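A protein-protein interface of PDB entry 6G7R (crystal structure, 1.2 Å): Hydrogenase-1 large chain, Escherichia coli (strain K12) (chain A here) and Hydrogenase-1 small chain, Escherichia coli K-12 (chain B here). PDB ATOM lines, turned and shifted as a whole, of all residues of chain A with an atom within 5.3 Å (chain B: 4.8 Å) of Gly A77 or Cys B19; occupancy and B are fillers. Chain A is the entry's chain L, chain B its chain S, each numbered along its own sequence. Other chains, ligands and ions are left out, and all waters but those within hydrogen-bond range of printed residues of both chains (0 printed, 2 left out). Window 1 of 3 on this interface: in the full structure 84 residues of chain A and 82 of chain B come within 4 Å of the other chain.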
ATOM      1  N   GLU A  73     -12.004  13.180   2.764  1.00  0.00           N
ATOM      2  CA  GLU A  73     -12.731  14.000   1.799  1.00  0.00           C
ATOM      3  C   GLU A  73     -12.608  15.484   2.135  1.00  0.00           C
ATOM      4  O   GLU A  73     -12.564  16.326   1.250  1.00  0.00           O
ATOM      5  CB  GLU A  73     -14.191  13.557   1.686  1.00  0.00           C
ATOM      6  CG  GLU A  73     -14.889  14.148   0.460  1.00  0.00           C
ATOM      7  CD  GLU A  73     -16.190  13.495   0.101  1.00  0.00           C
ATOM      8  OE1 GLU A  73     -17.031  13.345   1.040  1.00  0.00           O
ATOM      9  OE2 GLU A  73     -16.391  13.159  -1.062  1.00  0.00           O
ATOM     10  N   ILE A  75     -10.123  17.010   3.222  1.00  0.00           N
ATOM     11  CA  ILE A  75      -8.910  17.699   2.794  1.00  0.00           C
ATOM     12  C   ILE A  75      -9.287  18.885   1.912  1.00  0.00           C
ATOM     13  O   ILE A  75      -8.624  19.917   1.994  1.00  0.00           O
ATOM     14  CB  ILE A  75      -7.942  16.720   2.109  1.00  0.00           C
ATOM     15  CG1 ILE A  75      -7.326  15.782   3.152  1.00  0.00           C
ATOM     16  CG2 ILE A  75      -6.857  17.486   1.359  1.00  0.00           C
ATOM     17  CD1 ILE A  75      -6.551  14.651   2.588  1.00  0.00           C
ATOM     18  N   CYS A  76     -10.330  18.744   1.092  1.00  0.00           N
ATOM     19  CA  CYS A  76     -10.595  19.791   0.126  1.00  0.00           C
ATOM     20  C   CYS A  76     -12.042  19.722  -0.361  1.00  0.00           C
ATOM     21  O   CYS A  76     -12.519  18.683  -0.806  1.00  0.00           O
ATOM     22  CB  CYS A  76      -9.657  19.684  -1.070  1.00  0.00           C
ATOM     23  SG  CYS A  76      -9.813  21.106  -2.166  1.00  0.00           S
ATOM     24  N   GLY A  77     -12.716  20.875  -0.292  1.00  0.00           N
ATOM     25  CA  GLY A  77     -14.089  21.030  -0.793  1.00  0.00           C
ATOM     26  C   GLY A  77     -14.175  21.511  -2.236  1.00  0.00           C
ATOM     27  O   GLY A  77     -15.271  21.538  -2.779  1.00  0.00           O
ATOM     28  N   VAL A  78     -13.023  21.835  -2.824  1.00  0.00           N
ATOM     29  CA  VAL A  78     -12.933  22.226  -4.228  1.00  0.00           C
ATOM     30  C   VAL A  78     -12.795  20.947  -5.052  1.00  0.00           C
ATOM     31  O   VAL A  78     -13.671  20.635  -5.883  1.00  0.00           O
ATOM     32  CB  VAL A  78     -11.825  23.262  -4.481  1.00  0.00           C
ATOM     33  CG1 VAL A  78     -11.773  23.616  -5.955  1.00  0.00           C
ATOM     34  CG2 VAL A  78     -12.043  24.509  -3.622  1.00  0.00           C
ATOM     35  N   CYS A  79     -11.748  20.191  -4.785  1.00  0.00           N
ATOM     36  CA  CYS A  79     -11.606  18.878  -5.395  1.00  0.00           C
ATOM     37  C   CYS A  79     -12.383  17.829  -4.577  1.00  0.00           C
ATOM     38  O   CYS A  79     -11.882  16.764  -4.212  1.00  0.00           O
ATOM     39  CB  CYS A  79     -10.158  18.527  -5.678  1.00  0.00           C
ATOM     40  SG  CYS A  79      -9.054  18.482  -4.232  1.00  0.00           S
ATOM     41  N   THR A  80     -13.616  18.167  -4.248  1.00  0.00           N
ATOM     42  CA  THR A  80     -14.408  17.339  -3.365  1.00  0.00           C
ATOM     43  C   THR A  80     -14.772  16.002  -4.035  1.00  0.00           C
ATOM     44  O   THR A  80     -15.299  15.899  -5.133  1.00  0.00           O
ATOM     45  CB  THR A  80     -15.687  18.068  -2.960  1.00  0.00           C
ATOM     46  OG1 THR A  80     -16.401  17.241  -2.043  1.00  0.00           O
ATOM     47  CG2 THR A  80     -16.629  18.393  -4.101  1.00  0.00           C
ATOM     48  N   PRO A 228     -21.164  20.059  -1.963  1.00  0.00           N
ATOM     49  CA  PRO A 228     -19.891  19.354  -1.715  1.00  0.00           C
ATOM     50  C   PRO A 228     -19.986  18.141  -0.786  1.00  0.00           C
ATOM     51  O   PRO A 228     -20.932  17.997  -0.010  1.00  0.00           O
ATOM     52  CB  PRO A 228     -19.016  20.425  -1.068  1.00  0.00           C
ATOM     53  CG  PRO A 228     -19.562  21.738  -1.620  1.00  0.00           C
ATOM     54  CD  PRO A 228     -21.045  21.496  -1.681  1.00  0.00           C
ATOM     55  N   HIS A 229     -18.954  17.312  -0.902  1.00  0.00           N
ATOM     56  CA  HIS A 229     -18.660  16.210   0.038  1.00  0.00           C
ATOM     57  C   HIS A 229     -19.707  15.100  -0.023  1.00  0.00           C
ATOM     58  O   HIS A 229     -20.384  14.789   0.975  1.00  0.00           O
ATOM     59  CB  HIS A 229     -18.421  16.700   1.467  1.00  0.00           C
ATOM     60  CG  HIS A 229     -17.200  17.542   1.649  1.00  0.00           C
ATOM     61  ND1 HIS A 229     -16.094  17.436   0.792  1.00  0.00           N
ATOM     62  CD2 HIS A 229     -16.936  18.497   2.576  1.00  0.00           C
ATOM     63  CE1 HIS A 229     -15.180  18.265   1.241  1.00  0.00           C
ATOM     64  NE2 HIS A 229     -15.639  18.894   2.344  1.00  0.00           N
ATOM     65  N   CYS B  17     -11.494  23.824   4.225  1.00  0.00           N
ATOM     66  CA  CYS B  17     -11.366  23.093   2.978  1.00  0.00           C
ATOM     67  C   CYS B  17     -12.057  23.827   1.828  1.00  0.00           C
ATOM     68  O   CYS B  17     -11.973  23.351   0.698  1.00  0.00           O
ATOM     69  CB  CYS B  17     -11.897  21.668   3.156  1.00  0.00           C
ATOM     70  SG  CYS B  17     -13.677  21.496   2.890  1.00  0.00           S
ATOM     71  N   THR B  18     -12.805  24.910   2.122  1.00  0.00           N
ATOM     72  CA  THR B  18     -13.532  25.738   1.148  1.00  0.00           C
ATOM     73  C   THR B  18     -14.866  25.087   0.777  1.00  0.00           C
ATOM     74  O   THR B  18     -15.541  25.580  -0.125  1.00  0.00           O
ATOM     75  CB  THR B  18     -12.645  26.153  -0.035  1.00  0.00           C
ATOM     76  OG1 THR B  18     -11.433  26.666   0.521  1.00  0.00           O
ATOM     77  CG2 THR B  18     -13.275  27.254  -0.868  1.00  0.00           C
ATOM     78  N   CYS B  19     -15.276  24.057   1.482  1.00  0.00           N
ATOM     79  CA  CYS B  19     -16.598  23.472   1.197  1.00  0.00           C
ATOM     80  C   CYS B  19     -17.745  24.457   1.411  1.00  0.00           C
ATOM     81  O   CYS B  19     -18.795  24.335   0.788  1.00  0.00           O
ATOM     82  CB  CYS B  19     -16.889  22.153   1.930  1.00  0.00           C
ATOM     83  SG  CYS B  19     -16.980  22.055   3.762  1.00  0.00           S
ATOM     84  N   CYS B  20     -17.559  25.388   2.341  1.00  0.00           N
ATOM     85  CA  CYS B  20     -18.643  26.331   2.641  1.00  0.00           C
ATOM     86  C   CYS B  20     -18.823  27.397   1.538  1.00  0.00           C
ATOM     87  O   CYS B  20     -19.951  27.684   1.118  1.00  0.00           O
ATOM     88  CB  CYS B  20     -18.480  26.894   4.044  1.00  0.00           C
ATOM     89  SG  CYS B  20     -18.567  25.629   5.348  1.00  0.00           S
ATOM     90  N   THR B  21     -17.729  27.923   1.003  1.00  0.00           N
ATOM     91  CA  THR B  21     -17.800  28.802  -0.166  1.00  0.00           C
ATOM     92  C   THR B  21     -18.383  28.027  -1.347  1.00  0.00           C
ATOM     93  O   THR B  21     -19.198  28.565  -2.111  1.00  0.00           O
ATOM     94  CB  THR B  21     -16.400  29.315  -0.535  1.00  0.00           C
ATOM     95  OG1 THR B  21     -16.000  30.352   0.367  1.00  0.00           O
ATOM     96  CG2 THR B  21     -16.276  29.859  -1.943  1.00  0.00           C
ATOM     97  N   GLU B  22     -17.906  26.806  -1.559  1.00  0.00           N
ATOM     98  CA  GLU B  22     -18.425  26.002  -2.677  1.00  0.00           C
ATOM     99  C   GLU B  22     -19.919  25.785  -2.498  1.00  0.00           C
ATOM    100  O   GLU B  22     -20.647  25.889  -3.485  1.00  0.00           O
ATOM    101  CB  GLU B  22     -17.639  24.696  -2.811  1.00  0.00           C
ATOM    102  CG  GLU B  22     -16.236  24.866  -3.365  1.00  0.00           C
ATOM    103  CD  GLU B  22     -16.141  25.071  -4.881  1.00  0.00           C
ATOM    104  OE1 GLU B  22     -17.102  25.016  -5.639  1.00  0.00           O
ATOM    105  OE2 GLU B  22     -14.999  25.232  -5.358  1.00  0.00           O
ATOM    106  N   SER B  23     -20.376  25.469  -1.308  1.00  0.00           N
ATOM    107  CA  SER B  23     -21.803  25.300  -1.091  1.00  0.00           C
ATOM    108  C   SER B  23     -22.571  26.575  -1.453  1.00  0.00           C
ATOM    109  O   SER B  23     -23.582  26.549  -2.153  1.00  0.00           O
ATOM    110  CB  SER B  23     -22.071  24.881   0.321  1.00  0.00           C
ATOM    111  OG  SER B  23     -23.452  24.638   0.456  1.00  0.00           O
ATOM    112  N   GLU B  76     -15.380  31.552   7.352  1.00  0.00           N
ATOM    113  CA  GLU B  76     -15.252  30.155   6.949  1.00  0.00           C
ATOM    114  C   GLU B  76     -13.958  29.621   7.556  1.00  0.00           C
ATOM    115  O   GLU B  76     -12.953  30.322   7.536  1.00  0.00           O
ATOM    116  CB  GLU B  76     -15.250  30.086   5.427  1.00  0.00           C
ATOM    117  CG  GLU B  76     -15.102  28.710   4.802  1.00  0.00           C
ATOM    118  CD  GLU B  76     -15.395  28.714   3.313  1.00  0.00           C
ATOM    119  OE1 GLU B  76     -15.489  27.635   2.709  1.00  0.00           O
ATOM    120  OE2 GLU B  76     -15.724  29.818   2.792  1.00  0.00           O
ATOM    121  N   CYS B 149     -21.275  20.338   7.128  1.00  0.00           N
ATOM    122  CA  CYS B 149     -19.999  20.174   6.462  1.00  0.00           C
ATOM    123  C   CYS B 149     -20.236  19.802   4.991  1.00  0.00           C
ATOM    124  O   CYS B 149     -20.084  18.632   4.608  1.00  0.00           O
ATOM    125  CB  CYS B 149     -19.129  19.166   7.206  1.00  0.00           C
ATOM    126  SG  CYS B 149     -17.449  19.166   6.512  1.00  0.00           S
ATOM    127  N   PRO B 150     -20.541  20.779   4.141  1.00  0.00           N
ATOM    128  CA  PRO B 150     -20.916  22.147   4.475  1.00  0.00           C
ATOM    129  C   PRO B 150     -22.418  22.256   4.761  1.00  0.00           C
ATOM    130  O   PRO B 150     -23.164  21.264   4.617  1.00  0.00           O
ATOM    131  CB  PRO B 150     -20.610  22.899   3.153  1.00  0.00           C
ATOM    132  CG  PRO B 150     -20.933  21.882   2.078  1.00  0.00           C
ATOM    133  CD  PRO B 150     -20.692  20.524   2.703  1.00  0.00           C
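A ring nitrogen (NE2) of His A229 lies close to the side-chain sulfur (SG) of Cys B19 (3.7 Å). The side-chain sulfur (SG) of Cys B17 sits close to a ring nitrogen (NE2) of His A229 (3.3 Å). The backbone NH (N) of Gly A77 lies within hydrogen-bond range of the backbone carbonyl oxygen (O) of Cys B17.
The side-chain hydroxyl of Thr A80 is in hydrogen-bond range of the backbone NH of His A229, at 2.8 Å. The backbone NH (N) of Val A78 lies close to the side-chain sulfur (SG) of Cys A76, at 3.4 Å.
Among the printed residues, merely in contact across the chains: Val A78 with Glu B22 (3.5 Å), Gly A77 with Glu B22 (3.5 Å), Pro A228 with Cys B19 (3.6 Å), Pro A228 with Pro B150 (3.7 Å), Pro A228 with Glu B22 (3.7 Å), His A229 with Cys B149 (3.7 Å), Cys A76 with Cys B17 (3.8 Å), Pro A228 with Ser B23 (3.8 Å), Ile A75 with Cys B17 (3.9 Å), Gly A77 with Cys B19 (3.97 Å), Val A78 with Cys B17 (3.98 Å) and Val A78 with Thr B18 (3.99 Å).
Cys B19 touches just these residues of chain A: Gly A77, Pro A228 and His A229. Of the printed residues of chain B, Pro A228 touches Cys B19 (3.6 Å), Glu B22 (3.7 Å), Ser B23 (3.8 Å) and Pro B150 (3.7 Å). Of the printed residues of chain A, Thr B18 touches Val A78 (3.99 Å). Printed residues of chain A within 4 Å of Pro B150: Pro A228. Cys A79 touches none of the printed residues of chain B. The nearest residue of chain B that does not touch Gly A77 is Thr B18 (4.4 Å). The nearest printed residue of chain B that does not touch Cys A76 is Cys B19 (5.7 Å).
Hydrophobic or aromatic side chains of chain B within 4 Å of the printed part of chain A: Pro B150. Of the 9 printed residues of chain A, 6 touch a printed residue of chain B. Hydrophobic or aromatic side chains of chain A within 4 Å of the printed part of chain B: Val A78, Pro A228 and His A229. Along chain A the printed residues that touch a printed residue of chain B span positions 75 to 229. Among the printed residues, 15 pairs touch across the chains. Among the printed residues, no Asp or Glu carboxylate lies within 4 Å of a Lys or Arg side-chain nitrogen of the other chain.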
